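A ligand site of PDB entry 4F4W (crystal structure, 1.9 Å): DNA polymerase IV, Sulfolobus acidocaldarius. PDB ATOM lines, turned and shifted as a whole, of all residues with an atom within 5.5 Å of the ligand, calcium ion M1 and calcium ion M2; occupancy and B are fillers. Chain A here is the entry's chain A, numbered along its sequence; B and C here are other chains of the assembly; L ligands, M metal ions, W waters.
N4 of DC 13 of chain C sits close to a nitrogen (N3) of the ligand (3.4 Å).
The backbone NH (N) of Phe 12 is in hydrogen-bond range of an oxygen (O3) of the ligand, 3.3 Å away.
O11 of the ligand is in hydrogen-bond range of OH of Tyr 48.
A nitrogen (N3) of the ligand is in hydrogen-bond range of O6 of DG 5 of chain B, 2.9 Å away.
An oxygen (O9) of the ligand sits at hydrogen-bond distance from the side-chain hydroxyl (OG1) of Thr 45 (2.6 Å).
O11 of the ligand lies within hydrogen-bond range of N of Tyr 10.
NZ of Lys 160 is in salt-bridge range of O12 of the ligand (3.7 Å).
O12 of the ligand lies within salt-bridge range of NH1 of Arg 51, at 3.0 Å.
N of Phe 11 is in hydrogen-bond range of O3 of the ligand (3.4 Å).
OP1 of DC 13 of chain C is in salt-bridge range of NZ of Lys 153, at 3.8 Å.
The side-chain hydroxyl (OG) of Ser 103 sits close to the backbone NH (N) of Asp 105, 3.2 Å away.
OD1 of Asp 7 lies close to NZ of Lys 160 (3.4 Å).
The guanidinium group (NE) of Arg 51 is in hydrogen-bond range of the backbone carbonyl oxygen (O) of Ala 46 (2.9 Å).
The guanidinium group of Arg 51 is in hydrogen-bond range of the side-chain hydroxyl of Thr 45, 3.3 Å away.
The side-chain amino group (NZ) of Lys 153 lies within salt-bridge range of the side-chain carboxylate (OE2) of Glu 106 (2.6 Å).
CA of Asp 9 touches O11 of the ligand (3.6 Å).
Ala 44 touches the ligand (O to C1, 3.5 Å).
Ala 57 touches the ligand.
DG 6 of chain B touches the ligand.
Within 4 Å of the ligand: Asp 7, Phe 8, Asp 9, Tyr 10, Phe 11, Phe 12, Ala 44, Thr 45, Tyr 48, Arg 51, Ala 57, Asp 105, Lys 160, DG 5 of chain B, DG 6 of chain B and DC 13 of chain C.
The nearest printed residue that does not touch the ligand is Gly 58 (4.1 Å).
The nearest printed residue that does not touch calcium ion M1 is Lys 160 (4.1 Å).
Of the 25 residues printed, 4 come within 4 Å of calcium ion M2.
The nearest printed residue that does not touch calcium ion M2 is Ser 103 (4.6 Å).
Calcium ion M1 is bound by OD2 of Asp 7, O13 of the ligand, O of Phe 8, OD2 of Asp 105, O8 of the ligand and O6 of the ligand.
Calcium ion M1 has six donor atoms within binding distance.
Water W6 binds calcium ion M2 (2.1 Å).
An oxygen (O6) of the ligand binds calcium ion M2 (2.4 Å).
Calcium ion M2 is bound by OE1 of Glu 106.
Calcium ion M2 is bound by O3' of DC 13 of chain C, at 2.8 Å.
OD1 of Asp 7 is bound to calcium ion M2, 2.8 Å away.
The side-chain carboxylate (OD1) of Asp 105 is bound to calcium ion M2.
Slightly farther from calcium ion M2 lies the side-chain carboxylate (OD2) of Asp 7 (3.1 Å).
Water W2 lies within hydrogen-bond range of O1 of the ligand (2.7 Å) and N2 of DG 6 of chain B (3.3 Å).
Water W8 lies within hydrogen-bond range of OD2 of Asp 9 (3.1 Å), O of Asp 7 (3.2 Å) and O11 of the ligand (3.4 Å).
Water W7 lies within hydrogen-bond range of the side-chain hydroxyl (OG1) of Thr 45 (2.5 Å), the backbone carbonyl oxygen (O) of Ala 44 (3.0 Å) and an oxygen (O9) of the ligand (3.1 Å).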
ATOM      1  N   ASP A   7       9.337   4.260 -10.748  1.00  0.00           N
ATOM      2  CA  ASP A   7      10.242   5.052 -11.559  1.00  0.00           C
ATOM      3  C   ASP A   7      11.429   5.416 -10.668  1.00  0.00           C
ATOM      4  O   ASP A   7      11.243   6.052  -9.624  1.00  0.00           O
ATOM      5  CB  ASP A   7       9.525   6.290 -12.048  1.00  0.00           C
ATOM      6  CG  ASP A   7      10.311   7.058 -13.108  1.00  0.00           C
ATOM      7  OD1 ASP A   7       9.710   7.559 -14.078  1.00  0.00           O
ATOM      8  OD2 ASP A   7      11.501   7.203 -12.954  1.00  0.00           O
ATOM      9  N   PHE A   8      12.640   4.969 -11.025  1.00  0.00           N
ATOM     10  CA  PHE A   8      13.781   5.082 -10.105  1.00  0.00           C
ATOM     11  C   PHE A   8      14.232   6.557 -10.025  1.00  0.00           C
ATOM     12  O   PHE A   8      14.289   7.230 -11.030  1.00  0.00           O
ATOM     13  CB  PHE A   8      14.969   4.202 -10.544  1.00  0.00           C
ATOM     14  CG  PHE A   8      14.614   2.756 -10.812  1.00  0.00           C
ATOM     15  CD1 PHE A   8      15.399   1.992 -11.673  1.00  0.00           C
ATOM     16  CD2 PHE A   8      13.522   2.164 -10.238  1.00  0.00           C
ATOM     17  CE1 PHE A   8      15.087   0.665 -11.948  1.00  0.00           C
ATOM     18  CE2 PHE A   8      13.208   0.828 -10.502  1.00  0.00           C
ATOM     19  CZ  PHE A   8      13.996   0.089 -11.362  1.00  0.00           C
ATOM     20  N   ASP A   9      14.581   7.084  -8.849  1.00  0.00           N
ATOM     21  CA  ASP A   9      14.957   8.504  -8.807  1.00  0.00           C
ATOM     22  C   ASP A   9      16.350   8.773  -9.413  1.00  0.00           C
ATOM     23  O   ASP A   9      17.293   8.060  -9.116  1.00  0.00           O
ATOM     24  CB  ASP A   9      14.951   9.042  -7.364  1.00  0.00           C
ATOM     25  CG  ASP A   9      13.585   8.978  -6.711  1.00  0.00           C
ATOM     26  OD1 ASP A   9      13.549   8.819  -5.469  1.00  0.00           O
ATOM     27  OD2 ASP A   9      12.566   9.062  -7.436  1.00  0.00           O
ATOM     28  N   TYR A  10      16.452   9.832 -10.231  1.00  0.00           N
ATOM     29  CA  TYR A  10      17.713  10.321 -10.848  1.00  0.00           C
ATOM     30  C   TYR A  10      18.667   9.183 -11.141  1.00  0.00           C
ATOM     31  O   TYR A  10      19.845   9.164 -10.701  1.00  0.00           O
ATOM     32  CB  TYR A  10      18.371  11.474 -10.043  1.00  0.00           C
ATOM     33  CG  TYR A  10      18.882  11.174  -8.629  1.00  0.00           C
ATOM     34  CD1 TYR A  10      20.239  11.104  -8.362  1.00  0.00           C
ATOM     35  CD2 TYR A  10      17.997  11.034  -7.562  1.00  0.00           C
ATOM     36  CE1 TYR A  10      20.708  10.864  -7.053  1.00  0.00           C
ATOM     37  CE2 TYR A  10      18.458  10.768  -6.266  1.00  0.00           C
ATOM     38  CZ  TYR A  10      19.801  10.685  -6.030  1.00  0.00           C
ATOM     39  OH  TYR A  10      20.254  10.462  -4.756  1.00  0.00           O
ATOM     40  N   PHE A  11      18.131   8.197 -11.875  1.00  0.00           N
ATOM     41  CA  PHE A  11      18.666   6.833 -11.808  1.00  0.00           C
ATOM     42  C   PHE A  11      20.182   6.678 -11.973  1.00  0.00           C
ATOM     43  O   PHE A  11      20.866   6.182 -11.048  1.00  0.00           O
ATOM     44  CB  PHE A  11      17.901   5.889 -12.740  1.00  0.00           C
ATOM     45  CG  PHE A  11      18.322   4.451 -12.605  1.00  0.00           C
ATOM     46  CD1 PHE A  11      18.491   3.865 -11.339  1.00  0.00           C
ATOM     47  CD2 PHE A  11      18.519   3.667 -13.737  1.00  0.00           C
ATOM     48  CE1 PHE A  11      18.890   2.533 -11.224  1.00  0.00           C
ATOM     49  CE2 PHE A  11      18.903   2.328 -13.612  1.00  0.00           C
ATOM     50  CZ  PHE A  11      19.089   1.766 -12.361  1.00  0.00           C
ATOM     51  N   PHE A  12      20.740   7.084 -13.112  1.00  0.00           N
ATOM     52  CA  PHE A  12      22.154   6.809 -13.344  1.00  0.00           C
ATOM     53  C   PHE A  12      23.040   7.510 -12.311  1.00  0.00           C
ATOM     54  O   PHE A  12      24.031   6.939 -11.857  1.00  0.00           O
ATOM     55  CB  PHE A  12      22.635   7.240 -14.749  1.00  0.00           C
ATOM     56  CG  PHE A  12      22.016   6.495 -15.890  1.00  0.00           C
ATOM     57  CD1 PHE A  12      21.057   5.496 -15.715  1.00  0.00           C
ATOM     58  CD2 PHE A  12      22.411   6.818 -17.186  1.00  0.00           C
ATOM     59  CE1 PHE A  12      20.495   4.860 -16.787  1.00  0.00           C
ATOM     60  CE2 PHE A  12      21.883   6.173 -18.250  1.00  0.00           C
ATOM     61  CZ  PHE A  12      20.905   5.189 -18.076  1.00  0.00           C
ATOM     62  N   ALA A  13      22.700   8.753 -11.950  1.00  0.00           N
ATOM     63  CA  ALA A  13      23.494   9.484 -10.963  1.00  0.00           C
ATOM     64  C   ALA A  13      23.368   8.837  -9.586  1.00  0.00           C
ATOM     65  O   ALA A  13      24.344   8.765  -8.841  1.00  0.00           O
ATOM     66  CB  ALA A  13      23.079  10.991 -10.897  1.00  0.00           C
ATOM     67  N   VAL A  43      24.708  15.378 -21.375  1.00  0.00           N
ATOM     68  CA  VAL A  43      24.406  14.918 -20.026  1.00  0.00           C
ATOM     69  C   VAL A  43      23.333  13.851 -20.125  1.00  0.00           C
ATOM     70  O   VAL A  43      22.301  14.082 -20.745  1.00  0.00           O
ATOM     71  CB  VAL A  43      23.848  16.073 -19.189  1.00  0.00           C
ATOM     72  CG1 VAL A  43      23.292  15.564 -17.858  1.00  0.00           C
ATOM     73  CG2 VAL A  43      24.937  17.114 -18.962  1.00  0.00           C
ATOM     74  N   ALA A  44      23.586  12.702 -19.508  1.00  0.00           N
ATOM     75  CA  ALA A  44      22.568  11.640 -19.394  1.00  0.00           C
ATOM     76  C   ALA A  44      21.628  11.954 -18.232  1.00  0.00           C
ATOM     77  O   ALA A  44      20.394  11.827 -18.342  1.00  0.00           O
ATOM     78  CB  ALA A  44      23.224  10.248 -19.173  1.00  0.00           C
ATOM     79  N   THR A  45      22.198  12.330 -17.091  1.00  0.00           N
ATOM     80  CA  THR A  45      21.368  12.793 -16.011  1.00  0.00           C
ATOM     81  C   THR A  45      22.198  13.462 -14.950  1.00  0.00           C
ATOM     82  O   THR A  45      23.437  13.322 -14.923  1.00  0.00           O
ATOM     83  CB  THR A  45      20.523  11.684 -15.450  1.00  0.00           C
ATOM     84  OG1 THR A  45      19.391  12.245 -14.744  1.00  0.00           O
ATOM     85  CG2 THR A  45      21.335  10.813 -14.528  1.00  0.00           C
ATOM     86  N   ALA A  46      21.511  14.199 -14.093  1.00  0.00           N
ATOM     87  CA  ALA A  46      22.185  14.900 -12.996  1.00  0.00           C
ATOM     88  C   ALA A  46      21.399  14.631 -11.742  1.00  0.00           C
ATOM     89  O   ALA A  46      20.177  14.462 -11.801  1.00  0.00           O
ATOM     90  CB  ALA A  46      22.215  16.382 -13.265  1.00  0.00           C
ATOM     91  N   TYR A  48      19.752  15.824  -8.059  1.00  0.00           N
ATOM     92  CA  TYR A  48      18.892  16.989  -7.839  1.00  0.00           C
ATOM     93  C   TYR A  48      19.702  18.238  -7.468  1.00  0.00           C
ATOM     94  O   TYR A  48      19.333  19.340  -7.859  1.00  0.00           O
ATOM     95  CB  TYR A  48      17.823  16.662  -6.797  1.00  0.00           C
ATOM     96  CG  TYR A  48      16.959  15.474  -7.192  1.00  0.00           C
ATOM     97  CD1 TYR A  48      16.548  15.300  -8.500  1.00  0.00           C
ATOM     98  CD2 TYR A  48      16.609  14.505  -6.262  1.00  0.00           C
ATOM     99  CE1 TYR A  48      15.765  14.217  -8.872  1.00  0.00           C
ATOM    100  CE2 TYR A  48      15.833  13.425  -6.622  1.00  0.00           C
ATOM    101  CZ  TYR A  48      15.420  13.297  -7.939  1.00  0.00           C
ATOM    102  OH  TYR A  48      14.644  12.208  -8.305  1.00  0.00           O
ATOM    103  N   ARG A  51      20.717  19.670 -10.656  1.00  0.00           N
ATOM    104  CA  ARG A  51      19.573  20.247 -11.331  1.00  0.00           C
ATOM    105  C   ARG A  51      19.230  21.647 -10.782  1.00  0.00           C
ATOM    106  O   ARG A  51      18.776  22.532 -11.505  1.00  0.00           O
ATOM    107  CB  ARG A  51      18.352  19.320 -11.244  1.00  0.00           C
ATOM    108  CG  ARG A  51      18.491  18.052 -12.087  1.00  0.00           C
ATOM    109  CD  ARG A  51      17.298  17.160 -11.949  1.00  0.00           C
ATOM    110  NE  ARG A  51      17.654  15.778 -12.264  1.00  0.00           N
ATOM    111  CZ  ARG A  51      16.773  14.803 -12.412  1.00  0.00           C
ATOM    112  NH1 ARG A  51      15.492  15.060 -12.262  1.00  0.00           N
ATOM    113  NH2 ARG A  51      17.189  13.570 -12.725  1.00  0.00           N
ATOM    114  N   ALA A  57      19.192  16.856 -18.298  1.00  0.00           N
ATOM    115  CA  ALA A  57      19.490  15.735 -19.207  1.00  0.00           C
ATOM    116  C   ALA A  57      19.431  16.233 -20.643  1.00  0.00           C
ATOM    117  O   ALA A  57      18.548  17.003 -20.984  1.00  0.00           O
ATOM    118  CB  ALA A  57      18.478  14.597 -19.015  1.00  0.00           C
ATOM    119  N   GLY A  58      20.363  15.772 -21.476  1.00  0.00           N
ATOM    120  CA  GLY A  58      20.363  16.110 -22.891  1.00  0.00           C
ATOM    121  C   GLY A  58      21.227  17.316 -23.191  1.00  0.00           C
ATOM    122  O   GLY A  58      21.596  17.579 -24.330  1.00  0.00           O
ATOM    123  N   MET A  76      29.386   7.949 -18.223  1.00  0.00           N
ATOM    124  CA  MET A  76      28.270   7.029 -18.104  1.00  0.00           C
ATOM    125  C   MET A  76      28.857   5.603 -18.059  1.00  0.00           C
ATOM    126  O   MET A  76      29.757   5.274 -18.830  1.00  0.00           O
ATOM    127  CB  MET A  76      27.327   7.262 -19.308  1.00  0.00           C
ATOM    128  CG  MET A  76      25.859   6.821 -19.089  1.00  0.00           C
ATOM    129  SD  MET A  76      24.927   6.585 -20.589  1.00  0.00           S
ATOM    130  CE  MET A  76      26.209   6.120 -21.794  1.00  0.00           C
ATOM    131  N   SER A 103      11.196   0.652 -19.388  1.00  0.00           N
ATOM    132  CA  SER A 103      12.466   1.264 -19.743  1.00  0.00           C
ATOM    133  C   SER A 103      13.480   0.788 -18.720  1.00  0.00           C
ATOM    134  O   SER A 103      13.136   0.015 -17.843  1.00  0.00           O
ATOM    135  CB  SER A 103      12.404   2.811 -19.749  1.00  0.00           C
ATOM    136  OG  SER A 103      12.530   3.401 -18.461  1.00  0.00           O
ATOM    137  N   ILE A 104      14.720   1.236 -18.836  1.00  0.00           N
ATOM    138  CA  ILE A 104      15.747   0.828 -17.883  1.00  0.00           C
ATOM    139  C   ILE A 104      15.404   1.235 -16.446  1.00  0.00           C
ATOM    140  O   ILE A 104      15.959   0.698 -15.476  1.00  0.00           O
ATOM    141  CB  ILE A 104      17.118   1.423 -18.271  1.00  0.00           C
ATOM    142  CG1 ILE A 104      18.209   0.751 -17.425  1.00  0.00           C
ATOM    143  CG2 ILE A 104      17.124   2.951 -18.162  1.00  0.00           C
ATOM    144  CD1 ILE A 104      19.584   1.125 -17.841  1.00  0.00           C
ATOM    145  N   ASP A 105      14.540   2.214 -16.265  1.00  0.00           N
ATOM    146  CA  ASP A 105      14.260   2.572 -14.883  1.00  0.00           C
ATOM    147  C   ASP A 105      12.812   2.715 -14.498  1.00  0.00           C
ATOM    148  O   ASP A 105      12.513   3.340 -13.482  1.00  0.00           O
ATOM    149  CB  ASP A 105      15.028   3.809 -14.447  1.00  0.00           C
ATOM    150  CG  ASP A 105      14.303   5.080 -14.784  1.00  0.00           C
ATOM    151  OD1 ASP A 105      13.577   5.111 -15.783  1.00  0.00           O
ATOM    152  OD2 ASP A 105      14.496   6.055 -14.061  1.00  0.00           O
ATOM    153  N   GLU A 106      11.909   2.110 -15.267  1.00  0.00           N
ATOM    154  CA  GLU A 106      10.521   2.139 -14.825  1.00  0.00           C
ATOM    155  C   GLU A 106       9.724   0.904 -15.246  1.00  0.00           C
ATOM    156  O   GLU A 106      10.004   0.271 -16.300  1.00  0.00           O
ATOM    157  CB  GLU A 106       9.864   3.448 -15.248  1.00  0.00           C
ATOM    158  CG  GLU A 106       9.613   3.585 -16.683  1.00  0.00           C
ATOM    159  CD  GLU A 106       9.158   4.982 -17.084  1.00  0.00           C
ATOM    160  OE1 GLU A 106       9.835   5.966 -16.790  1.00  0.00           O
ATOM    161  OE2 GLU A 106       8.106   5.104 -17.694  1.00  0.00           O
ATOM    162  N   LYS A 153       1.358   6.547 -13.608  1.00  0.00           N
ATOM    163  CA  LYS A 153       2.519   7.336 -14.032  1.00  0.00           C
ATOM    164  C   LYS A 153       2.362   8.798 -13.685  1.00  0.00           C
ATOM    165  O   LYS A 153       3.253   9.408 -13.115  1.00  0.00           O
ATOM    166  CB  LYS A 153       2.782   7.181 -15.538  1.00  0.00           C
ATOM    167  CG  LYS A 153       3.984   7.966 -16.040  1.00  0.00           C
ATOM    168  CD  LYS A 153       4.196   7.649 -17.501  1.00  0.00           C
ATOM    169  CE  LYS A 153       5.515   8.154 -17.996  1.00  0.00           C
ATOM    170  NZ  LYS A 153       6.578   7.237 -17.531  1.00  0.00           N
ATOM    171  N   LYS A 160       7.561  13.021  -7.285  1.00  0.00           N
ATOM    172  CA  LYS A 160       9.028  12.880  -7.256  1.00  0.00           C
ATOM    173  C   LYS A 160       9.631  13.977  -6.394  1.00  0.00           C
ATOM    174  O   LYS A 160       9.115  15.086  -6.351  1.00  0.00           O
ATOM    175  CB  LYS A 160       9.634  12.972  -8.663  1.00  0.00           C
ATOM    176  CG  LYS A 160       9.289  11.834  -9.604  1.00  0.00           C
ATOM    177  CD  LYS A 160      10.183  11.842 -10.892  1.00  0.00           C
ATOM    178  CE  LYS A 160       9.804  10.736 -11.903  1.00  0.00           C
ATOM    179  NZ  LYS A 160      10.477  10.811 -13.276  1.00  0.00           N
ATOM    180  P    DG B   5      28.626  15.093 -29.293  1.00  0.00           P
ATOM    181  OP1  DG B   5      30.121  15.104 -29.393  1.00  0.00           O
ATOM    182  OP2  DG B   5      27.781  15.106 -30.518  1.00  0.00           O
ATOM    183  O5'  DG B   5      28.336  13.856 -28.337  1.00  0.00           O
ATOM    184  C5'  DG B   5      27.045  13.679 -27.788  1.00  0.00           C
ATOM    185  C4'  DG B   5      27.077  12.318 -27.131  1.00  0.00           C
ATOM    186  O4'  DG B   5      25.919  12.125 -26.298  1.00  0.00           O
ATOM    187  C3'  DG B   5      26.998  11.189 -28.165  1.00  0.00           C
ATOM    188  O3'  DG B   5      27.691  10.079 -27.642  1.00  0.00           O
ATOM    189  C2'  DG B   5      25.480  11.001 -28.308  1.00  0.00           C
ATOM    190  C1'  DG B   5      25.049  11.100 -26.848  1.00  0.00           C
ATOM    191  N9   DG B   5      23.749  11.717 -26.554  1.00  0.00           N
ATOM    192  C8   DG B   5      23.196  12.843 -27.122  1.00  0.00           C
ATOM    193  N7   DG B   5      22.064  13.189 -26.549  1.00  0.00           N
ATOM    194  C5   DG B   5      21.896  12.237 -25.540  1.00  0.00           C
ATOM    195  C6   DG B   5      20.890  12.108 -24.558  1.00  0.00           C
ATOM    196  O6   DG B   5      19.892  12.836 -24.406  1.00  0.00           O
ATOM    197  N1   DG B   5      21.103  11.023 -23.697  1.00  0.00           N
ATOM    198  C2   DG B   5      22.173  10.170 -23.762  1.00  0.00           C
ATOM    199  N2   DG B   5      22.261   9.154 -22.850  1.00  0.00           N
ATOM    200  N3   DG B   5      23.123  10.313 -24.661  1.00  0.00           N
ATOM    201  C4   DG B   5      22.933  11.361 -25.510  1.00  0.00           C
ATOM    202  P    DG B   6      28.104   8.831 -28.577  1.00  0.00           P
ATOM    203  OP1  DG B   6      29.288   8.188 -27.966  1.00  0.00           O
ATOM    204  OP2  DG B   6      28.054   9.293 -29.985  1.00  0.00           O
ATOM    205  O5'  DG B   6      26.879   7.839 -28.361  1.00  0.00           O
ATOM    206  C5'  DG B   6      26.703   7.311 -27.080  1.00  0.00           C
ATOM    207  C4'  DG B   6      25.390   6.577 -27.002  1.00  0.00           C
ATOM    208  O4'  DG B   6      24.346   7.531 -26.826  1.00  0.00           O
ATOM    209  C3'  DG B   6      25.015   5.762 -28.265  1.00  0.00           C
ATOM    210  O3'  DG B   6      24.599   4.516 -27.721  1.00  0.00           O
ATOM    211  C2'  DG B   6      23.818   6.568 -28.823  1.00  0.00           C
ATOM    212  C1'  DG B   6      23.212   7.094 -27.501  1.00  0.00           C
ATOM    213  N9   DG B   6      22.248   8.187 -27.600  1.00  0.00           N
ATOM    214  C8   DG B   6      22.223   9.209 -28.507  1.00  0.00           C
ATOM    215  N7   DG B   6      21.207  10.014 -28.370  1.00  0.00           N
ATOM    216  C5   DG B   6      20.534   9.496 -27.293  1.00  0.00           C
ATOM    217  C6   DG B   6      19.368   9.951 -26.677  1.00  0.00           C
ATOM    218  O6   DG B   6      18.730  10.913 -27.035  1.00  0.00           O
ATOM    219  N1   DG B   6      18.956   9.146 -25.611  1.00  0.00           N
ATOM    220  C2   DG B   6      19.622   8.049 -25.183  1.00  0.00           C
ATOM    221  N2   DG B   6      19.092   7.378 -24.148  1.00  0.00           N
ATOM    222  N3   DG B   6      20.733   7.631 -25.761  1.00  0.00           N
ATOM    223  C4   DG B   6      21.130   8.375 -26.814  1.00  0.00           C
ATOM    224  P    DC C  13       9.365  10.059 -20.927  1.00  0.00           P
ATOM    225  OP1  DC C  13       8.330   9.183 -20.323  1.00  0.00           O
ATOM    226  OP2  DC C  13       9.569  11.500 -20.563  1.00  0.00           O
ATOM    227  O5'  DC C  13      10.744   9.275 -20.649  1.00  0.00           O
ATOM    228  C5'  DC C  13      10.790   7.838 -20.732  1.00  0.00           C
ATOM    229  C4'  DC C  13      12.277   7.483 -20.741  1.00  0.00           C
ATOM    230  O4'  DC C  13      12.908   8.176 -21.841  1.00  0.00           O
ATOM    231  C3'  DC C  13      12.934   8.059 -19.519  1.00  0.00           C
ATOM    232  O3'  DC C  13      12.966   7.062 -18.483  1.00  0.00           O
ATOM    233  C2'  DC C  13      14.273   8.618 -20.004  1.00  0.00           C
ATOM    234  C1'  DC C  13      14.280   8.297 -21.494  1.00  0.00           C
ATOM    235  N1   DC C  13      14.918   9.261 -22.469  1.00  0.00           N
ATOM    236  C2   DC C  13      16.084   8.901 -23.219  1.00  0.00           C
ATOM    237  O2   DC C  13      16.605   7.798 -23.030  1.00  0.00           O
ATOM    238  N3   DC C  13      16.612   9.792 -24.080  1.00  0.00           N
ATOM    239  C4   DC C  13      16.044  10.982 -24.263  1.00  0.00           C
ATOM    240  N4   DC C  13      16.563  11.846 -25.138  1.00  0.00           N
ATOM    241  C5   DC C  13      14.875  11.364 -23.524  1.00  0.00           C
ATOM    242  C6   DC C  13      14.368  10.474 -22.667  1.00  0.00           C
HETATM  243  N1  LIG L   1      18.475   9.208 -19.713  1.00  0.00           N
HETATM  244  C1  LIG L   1      19.361   9.470 -20.710  1.00  0.00           C
HETATM  245  N2  LIG L   1      19.240  10.518 -21.530  1.00  0.00           N
HETATM  246  C2  LIG L   1      18.209  11.362 -21.329  1.00  0.00           C
HETATM  247  C3  LIG L   1      17.285  11.152 -20.315  1.00  0.00           C
HETATM  248  C4  LIG L   1      17.433  10.047 -19.473  1.00  0.00           C
HETATM  249  O1  LIG L   1      20.408   8.656 -20.885  1.00  0.00           O
HETATM  250  N3  LIG L   1      18.031  12.516 -22.166  1.00  0.00           N
HETATM  251  C5  LIG L   1      18.650   8.083 -18.799  1.00  0.00           C
HETATM  252  C6  LIG L   1      19.310   8.567 -17.559  1.00  0.00           C
HETATM  253  C7  LIG L   1      18.195   8.614 -16.565  1.00  0.00           C
HETATM  254  C8  LIG L   1      17.360   7.532 -16.999  1.00  0.00           C
HETATM  255  O2  LIG L   1      17.386   7.581 -18.439  1.00  0.00           O
HETATM  256  O3  LIG L   1      18.618   8.492 -15.207  1.00  0.00           O
HETATM  257  C9  LIG L   1      15.975   7.717 -16.543  1.00  0.00           C
HETATM  258  O4  LIG L   1      15.373   8.874 -17.067  1.00  0.00           O
HETATM  259  P1  LIG L   1      14.337   9.722 -16.246  1.00  0.00           P
HETATM  260  O5  LIG L   1      13.545  10.556 -17.203  1.00  0.00           O
HETATM  261  O6  LIG L   1      13.414   8.838 -15.528  1.00  0.00           O
HETATM  262  O7  LIG L   1      15.120  10.665 -15.266  1.00  0.00           O
HETATM  263  P2  LIG L   1      15.919  10.375 -13.949  1.00  0.00           P
HETATM  264  O8  LIG L   1      15.776   9.016 -13.411  1.00  0.00           O
HETATM  265  O9  LIG L   1      17.375  10.619 -14.209  1.00  0.00           O
HETATM  266  O10 LIG L   1      15.442  11.493 -12.928  1.00  0.00           O
HETATM  267  P3  LIG L   1      13.986  11.520 -12.254  1.00  0.00           P
HETATM  268  O11 LIG L   1      14.220  11.461 -10.769  1.00  0.00           O
HETATM  269  O12 LIG L   1      13.432  12.865 -12.567  1.00  0.00           O
HETATM  270  O13 LIG L   1      13.069  10.381 -12.738  1.00  0.00           O
HETATM  271 CA    CA M   1      13.561   8.079 -13.147  1.00  0.00          CA
HETATM  272 CA    CA M   2      11.731   7.250 -16.007  1.00  0.00          CA
HETATM  273  O   HOH W   1      12.102  14.738 -11.021  1.00  0.00           O
HETATM  274  O   HOH W   2      20.938   6.137 -21.650  1.00  0.00           O
HETATM  275  O   HOH W   3      15.823  14.427 -21.858  1.00  0.00           O
HETATM  276  O   HOH W   4      12.937  14.269 -15.024  1.00  0.00           O
HETATM  277  O   HOH W   5      15.379  12.779 -18.070  1.00  0.00           O
HETATM  278  O   HOH W   6      10.701   8.978 -16.607  1.00  0.00           O
HETATM  279  O   HOH W   7      17.907  12.294 -16.787  1.00  0.00           O
HETATM  280  O   HOH W   8      11.864   9.050 -10.449  1.00  0.00           O
